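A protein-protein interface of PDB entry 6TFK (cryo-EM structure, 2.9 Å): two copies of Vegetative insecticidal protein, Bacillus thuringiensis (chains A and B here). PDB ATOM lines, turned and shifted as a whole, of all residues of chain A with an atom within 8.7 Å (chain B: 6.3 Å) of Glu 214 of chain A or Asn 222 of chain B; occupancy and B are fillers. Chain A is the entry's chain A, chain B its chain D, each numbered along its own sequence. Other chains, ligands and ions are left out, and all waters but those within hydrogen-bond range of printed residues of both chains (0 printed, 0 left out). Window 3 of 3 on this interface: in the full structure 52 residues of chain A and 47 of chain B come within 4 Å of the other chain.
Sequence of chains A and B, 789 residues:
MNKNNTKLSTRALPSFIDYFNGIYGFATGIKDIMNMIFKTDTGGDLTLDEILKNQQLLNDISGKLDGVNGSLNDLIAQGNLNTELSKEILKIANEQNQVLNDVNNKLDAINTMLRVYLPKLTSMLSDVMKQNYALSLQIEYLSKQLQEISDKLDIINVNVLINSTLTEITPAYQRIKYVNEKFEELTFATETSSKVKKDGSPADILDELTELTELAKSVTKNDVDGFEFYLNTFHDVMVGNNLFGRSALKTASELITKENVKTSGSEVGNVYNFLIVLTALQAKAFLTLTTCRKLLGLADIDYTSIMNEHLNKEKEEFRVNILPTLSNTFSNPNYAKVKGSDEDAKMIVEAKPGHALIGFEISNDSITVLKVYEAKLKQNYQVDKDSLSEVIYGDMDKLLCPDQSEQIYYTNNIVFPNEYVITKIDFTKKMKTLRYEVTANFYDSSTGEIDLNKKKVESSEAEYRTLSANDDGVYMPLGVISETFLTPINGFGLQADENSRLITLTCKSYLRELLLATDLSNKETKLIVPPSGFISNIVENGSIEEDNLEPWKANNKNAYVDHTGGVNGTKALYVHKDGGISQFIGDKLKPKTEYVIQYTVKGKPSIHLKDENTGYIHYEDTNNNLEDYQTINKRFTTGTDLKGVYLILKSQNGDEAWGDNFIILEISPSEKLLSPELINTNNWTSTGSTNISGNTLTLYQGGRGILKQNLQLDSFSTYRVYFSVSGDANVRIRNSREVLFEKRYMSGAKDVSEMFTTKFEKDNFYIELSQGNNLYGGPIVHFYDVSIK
OD1 of Asp 223 of chain B lies close to OG of Ser 218 of chain A (3.4 Å). OE2 of Glu 211 of chain A lies within salt-bridge range of NH2 of Arg 293 of chain B. OD1 of Asn 222 of chain B sits close to OE1 of Glu 211 of chain A (2.4 Å). The side-chain carboxylate (OE2) of Glu 228 of chain B lies within salt-bridge range of the side-chain amino group (NZ) of Lys 182 of chain A (2.8 Å). The backbone NH (N) of Val 224 of chain B lies within hydrogen-bond range of the side-chain hydroxyl (OG) of Ser 218 of chain A, at 3.2 Å.
3 positions are printed for both chains. Of the 10 pairs that touch across the chains among the printed residues, none has its exchanged pair printed and touching as well.
Hydrophobic or aromatic side chains of chain B within 4 Å of the printed part of chain A: Val 224. Along chain B the printed residues that touch a printed residue of chain A span positions 222 to 293. Hydrophobic or aromatic side chains of chain A within 4 Å of the printed part of chain B: Tyr 178 and Val 219.
OE2 of Glu 214 of chain A is in salt-bridge range of NZ of Lys 217 of chain A. The side-chain amino group (NZ) of Lys 221 of chain B lies within salt-bridge range of the side-chain carboxylate (OD2) of Asp 223 of chain B (3.0 Å).
Printed residues of chain B within 4 Å of Tyr 178 of chain A: Asp 223 (3.8 Å) and Glu 228 (3.6 Å). Printed residues of chain B within 4 Å of Lys 182 of chain A: Glu 228. Of the printed residues of chain B, Glu 211 of chain A touches Asn 222 and Arg 293. Glu 214 of chain A touches just one residue of chain B: Asn 222. Of the printed residues of chain B, Val 219 of chain A touches Val 224 (3.7 Å). Of the printed residues of chain A, Asn 222 of chain B touches Glu 211 (2.4 Å), Glu 214 (3.8 Å) and Ser 218 (3.9 Å). Printed residues of chain A within 4 Å of Arg 293 of chain B: Glu 211. The nearest residue of chain B that does not touch Glu 214 of chain A is Asp 223 of chain B (4.9 Å).
CE2 of Tyr 178 of chain A touches O of Asp 223 of chain B (3.8 Å). OH of Tyr 178 of chain A touches OE1 of Glu 228 of chain B, at 3.6 Å. Glu 214 of chain A touches Asn 222 of chain B. Ser 218 of chain A touches Asn 222 of chain B (CB to O, 3.9 Å). Val 219 of chain A touches Val 224 of chain B (CG2 to CG2, 3.7 Å).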
ATOM      1  N   TYR A 178      24.947 -24.337 -25.527  1.00  0.00           N
ATOM      2  CA  TYR A 178      23.831 -23.918 -26.370  1.00  0.00           C
ATOM      3  C   TYR A 178      22.727 -23.272 -25.540  1.00  0.00           C
ATOM      4  O   TYR A 178      22.232 -22.189 -25.878  1.00  0.00           O
ATOM      5  CB  TYR A 178      23.296 -25.121 -27.146  1.00  0.00           C
ATOM      6  CG  TYR A 178      22.026 -24.858 -27.918  1.00  0.00           C
ATOM      7  CD1 TYR A 178      22.052 -24.174 -29.124  1.00  0.00           C
ATOM      8  CD2 TYR A 178      20.803 -25.309 -27.450  1.00  0.00           C
ATOM      9  CE1 TYR A 178      20.895 -23.939 -29.834  1.00  0.00           C
ATOM     10  CE2 TYR A 178      19.642 -25.078 -28.153  1.00  0.00           C
ATOM     11  CZ  TYR A 178      19.693 -24.394 -29.343  1.00  0.00           C
ATOM     12  OH  TYR A 178      18.535 -24.164 -30.045  1.00  0.00           O
ATOM     13  N   LYS A 182      21.532 -19.341 -25.711  1.00  0.00           N
ATOM     14  CA  LYS A 182      20.184 -19.093 -26.199  1.00  0.00           C
ATOM     15  C   LYS A 182      19.268 -18.491 -25.141  1.00  0.00           C
ATOM     16  O   LYS A 182      18.095 -18.236 -25.430  1.00  0.00           O
ATOM     17  CB  LYS A 182      19.577 -20.391 -26.740  1.00  0.00           C
ATOM     18  CG  LYS A 182      18.309 -20.187 -27.549  1.00  0.00           C
ATOM     19  CD  LYS A 182      18.145 -21.261 -28.611  1.00  0.00           C
ATOM     20  CE  LYS A 182      18.897 -20.909 -29.882  1.00  0.00           C
ATOM     21  NZ  LYS A 182      18.260 -19.779 -30.614  1.00  0.00           N
ATOM     22  N   PHE A 183      19.768 -18.257 -23.930  1.00  0.00           N
ATOM     23  CA  PHE A 183      19.026 -17.592 -22.864  1.00  0.00           C
ATOM     24  C   PHE A 183      19.832 -16.435 -22.295  1.00  0.00           C
ATOM     25  O   PHE A 183      19.845 -16.196 -21.084  1.00  0.00           O
ATOM     26  CB  PHE A 183      18.656 -18.575 -21.755  1.00  0.00           C
ATOM     27  CG  PHE A 183      17.472 -19.432 -22.075  1.00  0.00           C
ATOM     28  CD1 PHE A 183      17.637 -20.713 -22.568  1.00  0.00           C
ATOM     29  CD2 PHE A 183      16.189 -18.958 -21.875  1.00  0.00           C
ATOM     30  CE1 PHE A 183      16.544 -21.501 -22.861  1.00  0.00           C
ATOM     31  CE2 PHE A 183      15.095 -19.741 -22.167  1.00  0.00           C
ATOM     32  CZ  PHE A 183      15.272 -21.014 -22.660  1.00  0.00           C
ATOM     33  N   ASP A 207       7.020 -13.752 -30.699  1.00  0.00           N
ATOM     34  CA  ASP A 207       7.657 -14.880 -31.372  1.00  0.00           C
ATOM     35  C   ASP A 207       8.821 -15.421 -30.549  1.00  0.00           C
ATOM     36  O   ASP A 207       8.878 -16.619 -30.246  1.00  0.00           O
ATOM     37  CB  ASP A 207       8.131 -14.463 -32.763  1.00  0.00           C
ATOM     38  CG  ASP A 207       7.004 -13.932 -33.623  1.00  0.00           C
ATOM     39  OD1 ASP A 207       5.851 -14.367 -33.424  1.00  0.00           O
ATOM     40  OD2 ASP A 207       7.271 -13.082 -34.497  1.00  0.00           O
ATOM     41  N   GLU A 208       9.767 -14.551 -30.188  1.00  0.00           N
ATOM     42  CA  GLU A 208      10.907 -14.996 -29.394  1.00  0.00           C
ATOM     43  C   GLU A 208      10.458 -15.522 -28.039  1.00  0.00           C
ATOM     44  O   GLU A 208      11.032 -16.484 -27.519  1.00  0.00           O
ATOM     45  CB  GLU A 208      11.912 -13.856 -29.217  1.00  0.00           C
ATOM     46  CG  GLU A 208      11.400 -12.687 -28.386  1.00  0.00           C
ATOM     47  CD  GLU A 208      12.432 -11.589 -28.220  1.00  0.00           C
ATOM     48  OE1 GLU A 208      13.534 -11.715 -28.795  1.00  0.00           O
ATOM     49  OE2 GLU A 208      12.142 -10.601 -27.513  1.00  0.00           O
ATOM     50  N   LEU A 209       9.427 -14.911 -27.452  1.00  0.00           N
ATOM     51  CA  LEU A 209       8.956 -15.370 -26.153  1.00  0.00           C
ATOM     52  C   LEU A 209       8.365 -16.769 -26.250  1.00  0.00           C
ATOM     53  O   LEU A 209       8.584 -17.600 -25.366  1.00  0.00           O
ATOM     54  CB  LEU A 209       7.927 -14.391 -25.594  1.00  0.00           C
ATOM     55  CG  LEU A 209       7.618 -14.559 -24.107  1.00  0.00           C
ATOM     56  CD1 LEU A 209       8.848 -14.248 -23.261  1.00  0.00           C
ATOM     57  CD2 LEU A 209       6.450 -13.678 -23.703  1.00  0.00           C
ATOM     58  N   THR A 210       7.631 -17.054 -27.326  1.00  0.00           N
ATOM     59  CA  THR A 210       7.083 -18.392 -27.516  1.00  0.00           C
ATOM     60  C   THR A 210       8.189 -19.403 -27.789  1.00  0.00           C
ATOM     61  O   THR A 210       8.151 -20.530 -27.278  1.00  0.00           O
ATOM     62  CB  THR A 210       6.076 -18.389 -28.666  1.00  0.00           C
ATOM     63  OG1 THR A 210       6.667 -17.784 -29.821  1.00  0.00           O
ATOM     64  CG2 THR A 210       4.817 -17.622 -28.293  1.00  0.00           C
ATOM     65  N   GLU A 211       9.179 -19.027 -28.601  1.00  0.00           N
ATOM     66  CA  GLU A 211      10.278 -19.949 -28.869  1.00  0.00           C
ATOM     67  C   GLU A 211      11.061 -20.260 -27.600  1.00  0.00           C
ATOM     68  O   GLU A 211      11.410 -21.420 -27.349  1.00  0.00           O
ATOM     69  CB  GLU A 211      11.205 -19.373 -29.939  1.00  0.00           C
ATOM     70  CG  GLU A 211      10.524 -19.098 -31.265  1.00  0.00           C
ATOM     71  CD  GLU A 211      10.022 -20.352 -31.956  1.00  0.00           C
ATOM     72  OE1 GLU A 211      10.152 -21.455 -31.386  1.00  0.00           O
ATOM     73  OE2 GLU A 211       9.493 -20.231 -33.081  1.00  0.00           O
ATOM     74  N   LEU A 212      11.300 -19.258 -26.761  1.00  0.00           N
ATOM     75  CA  LEU A 212      12.017 -19.490 -25.521  1.00  0.00           C
ATOM     76  C   LEU A 212      11.148 -20.143 -24.458  1.00  0.00           C
ATOM     77  O   LEU A 212      11.685 -20.812 -23.575  1.00  0.00           O
ATOM     78  CB  LEU A 212      12.597 -18.176 -24.985  1.00  0.00           C
ATOM     79  CG  LEU A 212      13.615 -17.485 -25.905  1.00  0.00           C
ATOM     80  CD1 LEU A 212      14.259 -16.285 -25.225  1.00  0.00           C
ATOM     81  CD2 LEU A 212      14.683 -18.459 -26.378  1.00  0.00           C
ATOM     82  N   THR A 213       9.822 -20.018 -24.548  1.00  0.00           N
ATOM     83  CA  THR A 213       8.957 -20.794 -23.666  1.00  0.00           C
ATOM     84  C   THR A 213       8.983 -22.268 -24.046  1.00  0.00           C
ATOM     85  O   THR A 213       9.031 -23.141 -23.171  1.00  0.00           O
ATOM     86  CB  THR A 213       7.528 -20.250 -23.717  1.00  0.00           C
ATOM     87  OG1 THR A 213       7.517 -18.885 -23.287  1.00  0.00           O
ATOM     88  CG2 THR A 213       6.614 -21.059 -22.820  1.00  0.00           C
ATOM     89  N   GLU A 214       8.967 -22.564 -25.347  1.00  0.00           N
ATOM     90  CA  GLU A 214       9.141 -23.944 -25.793  1.00  0.00           C
ATOM     91  C   GLU A 214      10.488 -24.492 -25.343  1.00  0.00           C
ATOM     92  O   GLU A 214      10.583 -25.621 -24.840  1.00  0.00           O
ATOM     93  CB  GLU A 214       9.017 -24.023 -27.313  1.00  0.00           C
ATOM     94  CG  GLU A 214       7.633 -23.707 -27.853  1.00  0.00           C
ATOM     95  CD  GLU A 214       6.584 -24.700 -27.394  1.00  0.00           C
ATOM     96  OE1 GLU A 214       6.959 -25.830 -27.017  1.00  0.00           O
ATOM     97  OE2 GLU A 214       5.385 -24.351 -27.408  1.00  0.00           O
ATOM     98  N   LEU A 215      11.549 -23.706 -25.518  1.00  0.00           N
ATOM     99  CA  LEU A 215      12.863 -24.134 -25.054  1.00  0.00           C
ATOM    100  C   LEU A 215      12.846 -24.412 -23.555  1.00  0.00           C
ATOM    101  O   LEU A 215      13.294 -25.470 -23.105  1.00  0.00           O
ATOM    102  CB  LEU A 215      13.912 -23.079 -25.400  1.00  0.00           C
ATOM    103  CG  LEU A 215      15.090 -23.549 -26.256  1.00  0.00           C
ATOM    104  CD1 LEU A 215      16.075 -22.415 -26.452  1.00  0.00           C
ATOM    105  CD2 LEU A 215      15.787 -24.753 -25.643  1.00  0.00           C
ATOM    106  N   ALA A 216      12.359 -23.455 -22.760  1.00  0.00           N
ATOM    107  CA  ALA A 216      12.248 -23.654 -21.320  1.00  0.00           C
ATOM    108  C   ALA A 216      11.521 -24.948 -20.987  1.00  0.00           C
ATOM    109  O   ALA A 216      11.959 -25.709 -20.117  1.00  0.00           O
ATOM    110  CB  ALA A 216      11.526 -22.465 -20.688  1.00  0.00           C
ATOM    111  N   LYS A 217      10.397 -25.209 -21.658  1.00  0.00           N
ATOM    112  CA  LYS A 217       9.698 -26.472 -21.451  1.00  0.00           C
ATOM    113  C   LYS A 217      10.620 -27.650 -21.731  1.00  0.00           C
ATOM    114  O   LYS A 217      10.590 -28.659 -21.019  1.00  0.00           O
ATOM    115  CB  LYS A 217       8.460 -26.547 -22.344  1.00  0.00           C
ATOM    116  CG  LYS A 217       7.336 -25.604 -21.951  1.00  0.00           C
ATOM    117  CD  LYS A 217       6.230 -25.604 -22.995  1.00  0.00           C
ATOM    118  CE  LYS A 217       5.091 -24.682 -22.601  1.00  0.00           C
ATOM    119  NZ  LYS A 217       4.079 -24.549 -23.684  1.00  0.00           N
ATOM    120  N   SER A 218      11.447 -27.536 -22.771  1.00  0.00           N
ATOM    121  CA  SER A 218      12.386 -28.605 -23.094  1.00  0.00           C
ATOM    122  C   SER A 218      13.543 -28.687 -22.106  1.00  0.00           C
ATOM    123  O   SER A 218      14.243 -29.704 -22.077  1.00  0.00           O
ATOM    124  CB  SER A 218      12.935 -28.411 -24.505  1.00  0.00           C
ATOM    125  OG  SER A 218      13.872 -29.423 -24.825  1.00  0.00           O
ATOM    126  N   VAL A 219      13.761 -27.648 -21.306  1.00  0.00           N
ATOM    127  CA  VAL A 219      14.877 -27.597 -20.370  1.00  0.00           C
ATOM    128  C   VAL A 219      14.474 -28.094 -18.989  1.00  0.00           C
ATOM    129  O   VAL A 219      15.227 -28.830 -18.350  1.00  0.00           O
ATOM    130  CB  VAL A 219      15.443 -26.162 -20.296  1.00  0.00           C
ATOM    131  CG1 VAL A 219      16.427 -26.034 -19.148  1.00  0.00           C
ATOM    132  CG2 VAL A 219      16.108 -25.784 -21.603  1.00  0.00           C
ATOM    133  N   THR A 220      13.295 -27.704 -18.516  1.00  0.00           N
ATOM    134  CA  THR A 220      12.816 -28.116 -17.204  1.00  0.00           C
ATOM    135  C   THR A 220      12.203 -29.510 -17.206  1.00  0.00           C
ATOM    136  O   THR A 220      11.815 -29.998 -16.141  1.00  0.00           O
ATOM    137  CB  THR A 220      11.786 -27.112 -16.685  1.00  0.00           C
ATOM    138  OG1 THR A 220      10.639 -27.115 -17.544  1.00  0.00           O
ATOM    139  CG2 THR A 220      12.380 -25.714 -16.646  1.00  0.00           C
ATOM    140  N   LYS A 221      12.108 -30.159 -18.363  1.00  0.00           N
ATOM    141  CA  LYS A 221      11.510 -31.484 -18.439  1.00  0.00           C
ATOM    142  C   LYS A 221      12.368 -32.484 -17.674  1.00  0.00           C
ATOM    143  O   LYS A 221      13.568 -32.612 -17.937  1.00  0.00           O
ATOM    144  CB  LYS A 221      11.363 -31.909 -19.896  1.00  0.00           C
ATOM    145  CG  LYS A 221      10.456 -33.106 -20.099  1.00  0.00           C
ATOM    146  CD  LYS A 221      10.502 -33.592 -21.535  1.00  0.00           C
ATOM    147  CE  LYS A 221       9.563 -34.764 -21.755  1.00  0.00           C
ATOM    148  NZ  LYS A 221       9.768 -35.395 -23.088  1.00  0.00           N
ATOM    149  N   CYS A 292      14.290 -20.366 -16.531  1.00  0.00           N
ATOM    150  CA  CYS A 292      13.283 -21.120 -17.268  1.00  0.00           C
ATOM    151  C   CYS A 292      12.154 -21.565 -16.351  1.00  0.00           C
ATOM    152  O   CYS A 292      10.973 -21.456 -16.708  1.00  0.00           O
ATOM    153  CB  CYS A 292      13.927 -22.328 -17.946  1.00  0.00           C
ATOM    154  SG  CYS A 292      14.933 -21.922 -19.383  1.00  0.00           S
ATOM    155  N   LEU A 295      10.024 -18.585 -15.789  1.00  0.00           N
ATOM    156  CA  LEU A 295       9.293 -18.194 -16.988  1.00  0.00           C
ATOM    157  C   LEU A 295       8.109 -19.111 -17.251  1.00  0.00           C
ATOM    158  O   LEU A 295       7.070 -18.656 -17.741  1.00  0.00           O
ATOM    159  CB  LEU A 295      10.236 -18.188 -18.192  1.00  0.00           C
ATOM    160  CG  LEU A 295       9.609 -17.912 -19.559  1.00  0.00           C
ATOM    161  CD1 LEU A 295       8.854 -16.593 -19.557  1.00  0.00           C
ATOM    162  CD2 LEU A 295      10.680 -17.913 -20.636  1.00  0.00           C
ATOM    163  N   LEU A 296       8.242 -20.401 -16.939  1.00  0.00           N
ATOM    164  CA  LEU A 296       7.129 -21.320 -17.145  1.00  0.00           C
ATOM    165  C   LEU A 296       6.075 -21.195 -16.055  1.00  0.00           C
ATOM    166  O   LEU A 296       4.902 -21.502 -16.296  1.00  0.00           O
ATOM    167  CB  LEU A 296       7.636 -22.760 -17.208  1.00  0.00           C
ATOM    168  CG  LEU A 296       8.566 -23.097 -18.374  1.00  0.00           C
ATOM    169  CD1 LEU A 296       9.012 -24.540 -18.276  1.00  0.00           C
ATOM    170  CD2 LEU A 296       7.886 -22.838 -19.708  1.00  0.00           C
ATOM    171  N   VAL B 219      12.061 -31.355 -36.892  1.00  0.00           N
ATOM    172  CA  VAL B 219      13.218 -30.522 -37.194  1.00  0.00           C
ATOM    173  C   VAL B 219      13.071 -29.124 -36.609  1.00  0.00           C
ATOM    174  O   VAL B 219      14.026 -28.577 -36.059  1.00  0.00           O
ATOM    175  CB  VAL B 219      13.442 -30.460 -38.721  1.00  0.00           C
ATOM    176  CG1 VAL B 219      14.477 -29.405 -39.064  1.00  0.00           C
ATOM    177  CG2 VAL B 219      13.873 -31.812 -39.250  1.00  0.00           C
ATOM    178  N   THR B 220      11.883 -28.535 -36.718  1.00  0.00           N
ATOM    179  CA  THR B 220      11.636 -27.196 -36.200  1.00  0.00           C
ATOM    180  C   THR B 220      11.359 -27.181 -34.704  1.00  0.00           C
ATOM    181  O   THR B 220      11.171 -26.099 -34.138  1.00  0.00           O
ATOM    182  CB  THR B 220      10.458 -26.560 -36.940  1.00  0.00           C
ATOM    183  OG1 THR B 220       9.266 -27.310 -36.676  1.00  0.00           O
ATOM    184  CG2 THR B 220      10.720 -26.541 -38.437  1.00  0.00           C
ATOM    185  N   LYS B 221      11.327 -28.338 -34.052  1.00  0.00           N
ATOM    186  CA  LYS B 221      11.038 -28.396 -32.625  1.00  0.00           C
ATOM    187  C   LYS B 221      12.170 -27.746 -31.841  1.00  0.00           C
ATOM    188  O   LYS B 221      13.336 -28.124 -31.992  1.00  0.00           O
ATOM    189  CB  LYS B 221      10.846 -29.844 -32.189  1.00  0.00           C
ATOM    190  CG  LYS B 221      10.228 -29.995 -30.813  1.00  0.00           C
ATOM    191  CD  LYS B 221      10.241 -31.442 -30.359  1.00  0.00           C
ATOM    192  CE  LYS B 221       9.595 -31.602 -28.995  1.00  0.00           C
ATOM    193  NZ  LYS B 221       9.807 -32.966 -28.439  1.00  0.00           N
ATOM    194  N   ASN B 222      11.828 -26.768 -31.004  1.00  0.00           N
ATOM    195  CA  ASN B 222      12.814 -26.067 -30.185  1.00  0.00           C
ATOM    196  C   ASN B 222      13.070 -26.889 -28.929  1.00  0.00           C
ATOM    197  O   ASN B 222      12.300 -26.835 -27.969  1.00  0.00           O
ATOM    198  CB  ASN B 222      12.327 -24.666 -29.835  1.00  0.00           C
ATOM    199  CG  ASN B 222      11.900 -23.877 -31.052  1.00  0.00           C
ATOM    200  OD1 ASN B 222      10.719 -23.826 -31.392  1.00  0.00           O
ATOM    201  ND2 ASN B 222      12.865 -23.257 -31.722  1.00  0.00           N
ATOM    202  N   ASP B 223      14.159 -27.653 -28.934  1.00  0.00           N
ATOM    203  CA  ASP B 223      14.559 -28.480 -27.805  1.00  0.00           C
ATOM    204  C   ASP B 223      16.046 -28.282 -27.548  1.00  0.00           C
ATOM    205  O   ASP B 223      16.749 -27.612 -28.309  1.00  0.00           O
ATOM    206  CB  ASP B 223      14.252 -29.960 -28.062  1.00  0.00           C
ATOM    207  CG  ASP B 223      12.776 -30.278 -27.964  1.00  0.00           C
ATOM    208  OD1 ASP B 223      11.983 -29.360 -27.668  1.00  0.00           O
ATOM    209  OD2 ASP B 223      12.407 -31.452 -28.179  1.00  0.00           O
ATOM    210  N   VAL B 224      16.529 -28.878 -26.456  1.00  0.00           N
ATOM    211  CA  VAL B 224      17.960 -28.848 -26.177  1.00  0.00           C
ATOM    212  C   VAL B 224      18.718 -29.672 -27.208  1.00  0.00           C
ATOM    213  O   VAL B 224      19.903 -29.423 -27.462  1.00  0.00           O
ATOM    214  CB  VAL B 224      18.232 -29.343 -24.746  1.00  0.00           C
ATOM    215  CG1 VAL B 224      19.726 -29.407 -24.479  1.00  0.00           C
ATOM    216  CG2 VAL B 224      17.549 -28.442 -23.731  1.00  0.00           C
ATOM    217  N   GLY B 226      17.674 -30.015 -30.500  1.00  0.00           N
ATOM    218  CA  GLY B 226      17.045 -29.693 -31.761  1.00  0.00           C
ATOM    219  C   GLY B 226      18.041 -29.600 -32.898  1.00  0.00           C
ATOM    220  O   GLY B 226      19.255 -29.657 -32.712  1.00  0.00           O
ATOM    221  N   GLU B 228      18.658 -26.997 -34.680  1.00  0.00           N
ATOM    222  CA  GLU B 228      19.433 -25.773 -34.520  1.00  0.00           C
ATOM    223  C   GLU B 228      20.590 -25.981 -33.553  1.00  0.00           C
ATOM    224  O   GLU B 228      21.674 -25.416 -33.739  1.00  0.00           O
ATOM    225  CB  GLU B 228      18.528 -24.640 -34.036  1.00  0.00           C
ATOM    226  CG  GLU B 228      19.218 -23.289 -33.953  1.00  0.00           C
ATOM    227  CD  GLU B 228      18.384 -22.252 -33.231  1.00  0.00           C
ATOM    228  OE1 GLU B 228      17.186 -22.510 -32.994  1.00  0.00           O
ATOM    229  OE2 GLU B 228      18.930 -21.181 -32.895  1.00  0.00           O
ATOM    230  N   ARG B 293      10.152 -24.977 -41.984  1.00  0.00           N
ATOM    231  CA  ARG B 293       9.326 -23.957 -41.345  1.00  0.00           C
ATOM    232  C   ARG B 293       8.202 -23.509 -42.270  1.00  0.00           C
ATOM    233  O   ARG B 293       7.057 -23.349 -41.835  1.00  0.00           O
ATOM    234  CB  ARG B 293      10.178 -22.762 -40.920  1.00  0.00           C
ATOM    235  CG  ARG B 293      11.137 -23.066 -39.783  1.00  0.00           C
ATOM    236  CD  ARG B 293      11.602 -21.803 -39.073  1.00  0.00           C
ATOM    237  NE  ARG B 293      10.503 -21.069 -38.450  1.00  0.00           N
ATOM    238  CZ  ARG B 293      10.018 -21.319 -37.236  1.00  0.00           C
ATOM    239  NH1 ARG B 293      10.523 -22.296 -36.495  1.00  0.00           N
ATOM    240  NH2 ARG B 293       9.019 -20.590 -36.762  1.00  0.00           N
ATOM    241  N   ILE B 301      12.005 -17.083 -39.639  1.00  0.00           N
ATOM    242  CA  ILE B 301      13.046 -16.603 -38.736  1.00  0.00           C
ATOM    243  C   ILE B 301      14.245 -16.030 -39.488  1.00  0.00           C
ATOM    244  O   ILE B 301      15.135 -15.445 -38.858  1.00  0.00           O
ATOM    245  CB  ILE B 301      13.484 -17.726 -37.770  1.00  0.00           C
ATOM    246  CG1 ILE B 301      12.278 -18.242 -36.976  1.00  0.00           C
ATOM    247  CG2 ILE B 301      14.553 -17.235 -36.787  1.00  0.00           C
ATOM    248  CD1 ILE B 301      12.627 -19.222 -35.866  1.00  0.00           C
ATOM    249  N   TYR B 303      17.035 -17.266 -41.446  1.00  0.00           N
ATOM    250  CA  TYR B 303      18.308 -17.859 -41.059  1.00  0.00           C
ATOM    251  C   TYR B 303      19.463 -17.423 -41.948  1.00  0.00           C
ATOM    252  O   TYR B 303      20.553 -17.996 -41.844  1.00  0.00           O
ATOM    253  CB  TYR B 303      18.201 -19.384 -41.068  1.00  0.00           C
ATOM    254  CG  TYR B 303      17.331 -19.923 -39.964  1.00  0.00           C
ATOM    255  CD1 TYR B 303      17.772 -19.921 -38.651  1.00  0.00           C
ATOM    256  CD2 TYR B 303      16.072 -20.435 -40.232  1.00  0.00           C
ATOM    257  CE1 TYR B 303      16.985 -20.412 -37.636  1.00  0.00           C
ATOM    258  CE2 TYR B 303      15.276 -20.927 -39.222  1.00  0.00           C
ATOM    259  CZ  TYR B 303      15.738 -20.913 -37.925  1.00  0.00           C
ATOM    260  OH  TYR B 303      14.955 -21.403 -36.909  1.00  0.00           O
